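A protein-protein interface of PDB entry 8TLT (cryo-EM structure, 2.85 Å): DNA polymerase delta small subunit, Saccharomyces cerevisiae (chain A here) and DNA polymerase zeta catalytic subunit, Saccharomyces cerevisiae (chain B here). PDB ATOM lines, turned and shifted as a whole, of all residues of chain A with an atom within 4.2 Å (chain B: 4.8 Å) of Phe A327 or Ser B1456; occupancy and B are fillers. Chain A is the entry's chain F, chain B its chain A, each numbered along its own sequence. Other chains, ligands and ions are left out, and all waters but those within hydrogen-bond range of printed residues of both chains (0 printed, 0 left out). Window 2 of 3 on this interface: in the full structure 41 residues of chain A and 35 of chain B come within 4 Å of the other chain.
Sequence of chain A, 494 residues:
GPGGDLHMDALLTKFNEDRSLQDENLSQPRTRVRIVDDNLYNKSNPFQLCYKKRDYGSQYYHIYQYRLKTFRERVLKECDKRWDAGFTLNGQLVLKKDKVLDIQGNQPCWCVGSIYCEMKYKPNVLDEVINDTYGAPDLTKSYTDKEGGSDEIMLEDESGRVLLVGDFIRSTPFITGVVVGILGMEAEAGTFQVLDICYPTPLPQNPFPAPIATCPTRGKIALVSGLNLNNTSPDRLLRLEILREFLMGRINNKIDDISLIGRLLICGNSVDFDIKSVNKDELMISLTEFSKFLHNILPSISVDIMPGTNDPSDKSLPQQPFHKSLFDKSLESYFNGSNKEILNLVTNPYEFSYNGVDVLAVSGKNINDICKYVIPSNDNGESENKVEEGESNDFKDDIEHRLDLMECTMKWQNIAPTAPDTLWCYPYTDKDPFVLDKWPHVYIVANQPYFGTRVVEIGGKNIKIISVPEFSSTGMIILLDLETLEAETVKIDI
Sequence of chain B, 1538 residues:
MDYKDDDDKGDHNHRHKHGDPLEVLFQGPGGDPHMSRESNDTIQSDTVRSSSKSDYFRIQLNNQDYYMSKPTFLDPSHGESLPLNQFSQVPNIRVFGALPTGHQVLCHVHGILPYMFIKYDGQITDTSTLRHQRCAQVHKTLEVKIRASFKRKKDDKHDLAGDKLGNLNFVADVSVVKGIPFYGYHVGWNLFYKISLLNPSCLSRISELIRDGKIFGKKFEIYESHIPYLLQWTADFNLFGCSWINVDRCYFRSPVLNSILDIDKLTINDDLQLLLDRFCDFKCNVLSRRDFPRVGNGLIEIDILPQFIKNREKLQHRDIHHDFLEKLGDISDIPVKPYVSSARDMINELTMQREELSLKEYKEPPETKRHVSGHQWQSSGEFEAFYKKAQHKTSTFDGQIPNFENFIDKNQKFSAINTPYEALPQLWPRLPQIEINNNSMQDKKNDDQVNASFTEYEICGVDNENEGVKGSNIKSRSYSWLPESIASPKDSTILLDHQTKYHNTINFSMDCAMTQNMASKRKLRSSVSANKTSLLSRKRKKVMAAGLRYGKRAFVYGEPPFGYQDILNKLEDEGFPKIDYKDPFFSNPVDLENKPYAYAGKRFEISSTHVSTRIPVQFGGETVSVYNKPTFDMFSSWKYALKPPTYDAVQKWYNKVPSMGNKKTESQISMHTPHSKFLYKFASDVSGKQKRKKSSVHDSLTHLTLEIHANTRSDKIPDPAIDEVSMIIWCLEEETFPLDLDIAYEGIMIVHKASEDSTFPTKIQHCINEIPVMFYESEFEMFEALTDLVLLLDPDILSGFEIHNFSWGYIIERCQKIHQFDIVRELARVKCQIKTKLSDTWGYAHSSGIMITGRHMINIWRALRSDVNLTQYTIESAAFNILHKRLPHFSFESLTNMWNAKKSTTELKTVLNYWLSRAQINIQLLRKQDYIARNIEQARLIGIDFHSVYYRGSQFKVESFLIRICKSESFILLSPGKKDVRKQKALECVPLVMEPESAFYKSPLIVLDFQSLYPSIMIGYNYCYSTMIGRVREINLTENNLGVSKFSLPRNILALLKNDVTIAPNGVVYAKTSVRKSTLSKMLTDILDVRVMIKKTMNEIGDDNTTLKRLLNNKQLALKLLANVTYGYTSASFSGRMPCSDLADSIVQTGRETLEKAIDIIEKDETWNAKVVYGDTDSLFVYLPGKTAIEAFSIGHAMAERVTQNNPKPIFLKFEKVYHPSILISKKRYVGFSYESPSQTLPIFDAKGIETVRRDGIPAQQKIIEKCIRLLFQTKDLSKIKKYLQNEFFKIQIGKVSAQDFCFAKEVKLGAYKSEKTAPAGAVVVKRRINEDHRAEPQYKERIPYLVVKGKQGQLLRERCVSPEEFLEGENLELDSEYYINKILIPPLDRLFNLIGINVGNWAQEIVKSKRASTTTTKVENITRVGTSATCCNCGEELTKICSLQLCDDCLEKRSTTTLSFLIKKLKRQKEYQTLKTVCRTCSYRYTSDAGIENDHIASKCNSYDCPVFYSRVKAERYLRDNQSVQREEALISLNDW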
ATOM      1  N   LEU A 294      28.474  19.964 -17.003  1.00  0.00           N
ATOM      2  CA  LEU A 294      27.660  18.926 -16.377  1.00  0.00           C
ATOM      3  C   LEU A 294      26.387  18.665 -17.171  1.00  0.00           C
ATOM      4  O   LEU A 294      26.000  17.511 -17.374  1.00  0.00           O
ATOM      5  CB  LEU A 294      27.320  19.318 -14.941  1.00  0.00           C
ATOM      6  CG  LEU A 294      28.413  19.105 -13.894  1.00  0.00           C
ATOM      7  CD1 LEU A 294      27.943  19.584 -12.533  1.00  0.00           C
ATOM      8  CD2 LEU A 294      28.816  17.644 -13.841  1.00  0.00           C
ATOM      9  N   HIS A 323      26.144  23.020  -2.428  1.00  0.00           N
ATOM     10  CA  HIS A 323      24.779  23.484  -2.254  1.00  0.00           C
ATOM     11  C   HIS A 323      23.975  23.246  -3.527  1.00  0.00           C
ATOM     12  O   HIS A 323      24.519  23.204  -4.632  1.00  0.00           O
ATOM     13  CB  HIS A 323      24.768  24.965  -1.885  1.00  0.00           C
ATOM     14  CG  HIS A 323      25.284  25.244  -0.507  1.00  0.00           C
ATOM     15  ND1 HIS A 323      24.539  25.016   0.629  1.00  0.00           N
ATOM     16  CD2 HIS A 323      26.474  25.733  -0.085  1.00  0.00           C
ATOM     17  CE1 HIS A 323      25.246  25.353   1.692  1.00  0.00           C
ATOM     18  NE2 HIS A 323      26.424  25.792   1.287  1.00  0.00           N
ATOM     19  N   LYS A 324      22.663  23.061  -3.358  1.00  0.00           N
ATOM     20  CA  LYS A 324      21.796  22.842  -4.511  1.00  0.00           C
ATOM     21  C   LYS A 324      21.819  24.033  -5.457  1.00  0.00           C
ATOM     22  O   LYS A 324      21.661  23.868  -6.671  1.00  0.00           O
ATOM     23  CB  LYS A 324      20.368  22.558  -4.047  1.00  0.00           C
ATOM     24  CG  LYS A 324      20.064  21.086  -3.851  1.00  0.00           C
ATOM     25  CD  LYS A 324      18.614  20.777  -4.169  1.00  0.00           C
ATOM     26  CE  LYS A 324      18.120  19.586  -3.369  1.00  0.00           C
ATOM     27  NZ  LYS A 324      18.238  19.818  -1.904  1.00  0.00           N
ATOM     28  N   SER A 325      22.024  25.234  -4.924  1.00  0.00           N
ATOM     29  CA  SER A 325      22.217  26.423  -5.740  1.00  0.00           C
ATOM     30  C   SER A 325      23.654  26.428  -6.254  1.00  0.00           C
ATOM     31  O   SER A 325      24.351  25.412  -6.215  1.00  0.00           O
ATOM     32  CB  SER A 325      21.871  27.675  -4.942  1.00  0.00           C
ATOM     33  OG  SER A 325      20.635  27.520  -4.267  1.00  0.00           O
ATOM     34  N   LEU A 326      24.107  27.572  -6.767  1.00  0.00           N
ATOM     35  CA  LEU A 326      25.420  27.687  -7.406  1.00  0.00           C
ATOM     36  C   LEU A 326      25.521  26.782  -8.630  1.00  0.00           C
ATOM     37  O   LEU A 326      26.615  26.384  -9.036  1.00  0.00           O
ATOM     38  CB  LEU A 326      26.560  27.390  -6.424  1.00  0.00           C
ATOM     39  CG  LEU A 326      26.594  28.189  -5.121  1.00  0.00           C
ATOM     40  N   PHE A 327      24.376  26.453  -9.219  1.00  0.00           N
ATOM     41  CA  PHE A 327      24.300  25.664 -10.437  1.00  0.00           C
ATOM     42  C   PHE A 327      23.304  26.324 -11.378  1.00  0.00           C
ATOM     43  O   PHE A 327      22.402  27.044 -10.943  1.00  0.00           O
ATOM     44  CB  PHE A 327      23.876  24.217 -10.149  1.00  0.00           C
ATOM     45  CG  PHE A 327      24.982  23.356  -9.605  1.00  0.00           C
ATOM     46  CD1 PHE A 327      25.973  22.871 -10.439  1.00  0.00           C
ATOM     47  CD2 PHE A 327      25.028  23.031  -8.262  1.00  0.00           C
ATOM     48  CE1 PHE A 327      26.991  22.078  -9.943  1.00  0.00           C
ATOM     49  CE2 PHE A 327      26.043  22.239  -7.760  1.00  0.00           C
ATOM     50  CZ  PHE A 327      27.023  21.763  -8.601  1.00  0.00           C
ATOM     51  N   ASP A 328      23.476  26.079 -12.673  1.00  0.00           N
ATOM     52  CA  ASP A 328      22.622  26.712 -13.664  1.00  0.00           C
ATOM     53  C   ASP A 328      21.187  26.209 -13.539  1.00  0.00           C
ATOM     54  O   ASP A 328      20.918  25.133 -12.998  1.00  0.00           O
ATOM     55  CB  ASP A 328      23.151  26.456 -15.074  1.00  0.00           C
ATOM     56  N   LYS A 329      20.254  27.017 -14.047  1.00  0.00           N
ATOM     57  CA  LYS A 329      18.840  26.664 -13.988  1.00  0.00           C
ATOM     58  C   LYS A 329      18.517  25.427 -14.813  1.00  0.00           C
ATOM     59  O   LYS A 329      17.466  24.812 -14.601  1.00  0.00           O
ATOM     60  CB  LYS A 329      17.985  27.841 -14.461  1.00  0.00           C
ATOM     61  CG  LYS A 329      18.183  29.113 -13.657  1.00  0.00           C
ATOM     62  N   LEU A 331      19.814  22.607 -14.569  1.00  0.00           N
ATOM     63  CA  LEU A 331      20.016  21.418 -13.753  1.00  0.00           C
ATOM     64  C   LEU A 331      18.888  21.192 -12.754  1.00  0.00           C
ATOM     65  O   LEU A 331      19.021  20.344 -11.862  1.00  0.00           O
ATOM     66  CB  LEU A 331      21.357  21.510 -13.019  1.00  0.00           C
ATOM     67  CG  LEU A 331      22.553  20.792 -13.648  1.00  0.00           C
ATOM     68  CD1 LEU A 331      22.817  21.302 -15.051  1.00  0.00           C
ATOM     69  CD2 LEU A 331      23.788  20.959 -12.782  1.00  0.00           C
ATOM     70  N   PHE A 335      18.218  18.165 -10.069  1.00  0.00           N
ATOM     71  CA  PHE A 335      18.158  18.482  -8.649  1.00  0.00           C
ATOM     72  C   PHE A 335      16.751  18.345  -8.077  1.00  0.00           C
ATOM     73  O   PHE A 335      16.470  18.885  -7.001  1.00  0.00           O
ATOM     74  CB  PHE A 335      18.697  19.891  -8.399  1.00  0.00           C
ATOM     75  CG  PHE A 335      20.191  19.992  -8.502  1.00  0.00           C
ATOM     76  CD1 PHE A 335      21.005  19.124  -7.796  1.00  0.00           C
ATOM     77  CD2 PHE A 335      20.780  20.949  -9.307  1.00  0.00           C
ATOM     78  CE1 PHE A 335      22.379  19.212  -7.890  1.00  0.00           C
ATOM     79  CE2 PHE A 335      22.153  21.041  -9.404  1.00  0.00           C
ATOM     80  CZ  PHE A 335      22.952  20.171  -8.695  1.00  0.00           C
ATOM     81  N   LEU A 345      25.801  14.696  -5.166  1.00  0.00           N
ATOM     82  CA  LEU A 345      26.716  15.577  -4.453  1.00  0.00           C
ATOM     83  C   LEU A 345      26.974  14.980  -3.076  1.00  0.00           C
ATOM     84  O   LEU A 345      26.032  14.764  -2.306  1.00  0.00           O
ATOM     85  CB  LEU A 345      26.144  16.990  -4.334  1.00  0.00           C
ATOM     86  CG  LEU A 345      26.348  18.003  -5.468  1.00  0.00           C
ATOM     87  CD1 LEU A 345      26.327  17.351  -6.836  1.00  0.00           C
ATOM     88  CD2 LEU A 345      25.298  19.097  -5.389  1.00  0.00           C
ATOM     89  N   LYS B1454      16.865  35.522  -6.411  1.00  0.00           N
ATOM     90  CA  LYS B1454      18.135  35.095  -6.998  1.00  0.00           C
ATOM     91  C   LYS B1454      18.907  34.310  -5.943  1.00  0.00           C
ATOM     92  O   LYS B1454      19.741  34.839  -5.205  1.00  0.00           O
ATOM     93  CB  LYS B1454      18.923  36.296  -7.507  1.00  0.00           C
ATOM     94  N   ARG B1455      18.607  33.010  -5.874  1.00  0.00           N
ATOM     95  CA  ARG B1455      19.221  32.158  -4.859  1.00  0.00           C
ATOM     96  C   ARG B1455      20.726  32.041  -5.062  1.00  0.00           C
ATOM     97  O   ARG B1455      21.489  32.018  -4.089  1.00  0.00           O
ATOM     98  CB  ARG B1455      18.577  30.772  -4.873  1.00  0.00           C
ATOM     99  CG  ARG B1455      17.116  30.753  -4.475  1.00  0.00           C
ATOM    100  CD  ARG B1455      16.544  29.350  -4.581  1.00  0.00           C
ATOM    101  NE  ARG B1455      16.628  28.828  -5.940  1.00  0.00           N
ATOM    102  CZ  ARG B1455      16.195  27.631  -6.310  1.00  0.00           C
ATOM    103  N   SER B1456      21.168  31.949  -6.318  1.00  0.00           N
ATOM    104  CA  SER B1456      22.580  31.703  -6.598  1.00  0.00           C
ATOM    105  C   SER B1456      23.456  32.840  -6.084  1.00  0.00           C
ATOM    106  O   SER B1456      24.478  32.603  -5.430  1.00  0.00           O
ATOM    107  CB  SER B1456      22.786  31.499  -8.097  1.00  0.00           C
ATOM    108  OG  SER B1456      22.628  30.138  -8.453  1.00  0.00           O
ATOM    109  N   THR B1457      23.070  34.085  -6.363  1.00  0.00           N
ATOM    110  CA  THR B1457      23.879  35.222  -5.933  1.00  0.00           C
ATOM    111  C   THR B1457      23.930  35.319  -4.413  1.00  0.00           C
ATOM    112  O   THR B1457      24.993  35.562  -3.827  1.00  0.00           O
ATOM    113  CB  THR B1457      23.331  36.515  -6.538  1.00  0.00           C
ATOM    114  N   THR B1458      22.784  35.130  -3.755  1.00  0.00           N
ATOM    115  CA  THR B1458      22.736  35.221  -2.298  1.00  0.00           C
ATOM    116  C   THR B1458      23.582  34.133  -1.649  1.00  0.00           C
ATOM    117  O   THR B1458      24.369  34.405  -0.730  1.00  0.00           O
ATOM    118  CB  THR B1458      21.287  35.133  -1.815  1.00  0.00           C
ATOM    119  N   THR B1459      23.430  32.888  -2.111  1.00  0.00           N
ATOM    120  CA  THR B1459      24.211  31.800  -1.535  1.00  0.00           C
ATOM    121  C   THR B1459      25.696  31.986  -1.815  1.00  0.00           C
ATOM    122  O   THR B1459      26.535  31.676  -0.962  1.00  0.00           O
ATOM    123  CB  THR B1459      23.711  30.443  -2.047  1.00  0.00           C
ATOM    124  OG1 THR B1459      24.339  29.389  -1.307  1.00  0.00           O
ATOM    125  CG2 THR B1459      24.015  30.244  -3.513  1.00  0.00           C
ATOM    126  N   LEU B1460      26.044  32.527  -2.986  1.00  0.00           N
ATOM    127  CA  LEU B1460      27.448  32.771  -3.290  1.00  0.00           C
ATOM    128  C   LEU B1460      28.034  33.838  -2.375  1.00  0.00           C
ATOM    129  O   LEU B1460      29.153  33.686  -1.877  1.00  0.00           O
ATOM    130  CB  LEU B1460      27.603  33.166  -4.757  1.00  0.00           C
ATOM    131  CG  LEU B1460      28.966  32.901  -5.393  1.00  0.00           C
ATOM    132  CD1 LEU B1460      29.577  31.626  -4.837  1.00  0.00           C
ATOM    133  CD2 LEU B1460      28.837  32.816  -6.901  1.00  0.00           C
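The side-chain hydroxyl of Ser B1456 is in hydrogen-bond range of the backbone NH of Leu A326.
Ser A325 touches Arg B1455.
Ser A325 touches Thr B1459 (CB to CG2, 3.6 Å).
Thr B1459 touches Leu A326.
OG of Ser B1456 touches O of Phe A327, at 3.98 Å.
Phe A327 touches just one residue of chain B: Ser B1456.
Ser B1456 touches two residues of chain A.
Printed residues of chain B within 4 Å of Leu A326: Ser B1456 and Thr B1459.
Of the printed residues of chain A, Arg B1455 touches Ser A325 (3.9 Å).
Of the printed residues of chain A, Thr B1459 touches Ser A325 and Leu A326.
Of the printed residues of chain B, Ser A325 touches Arg B1455 and Thr B1459.
Leu B1460 touches none of the printed residues of chain A.
Leu A331 touches none of the printed residues of chain B.
The nearest printed residue of chain B that does not touch Phe A327 is Thr B1459 (6.9 Å).
The nearest printed residue of chain B that does not touch Ser A325 is Ser B1456 (4.4 Å).
Of the 11 printed residues of chain A, 3 touch a printed residue of chain B.
Among the printed residues, no Asp or Glu carboxylate lies within 4 Å of a Lys or Arg side-chain nitrogen of the other chain.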
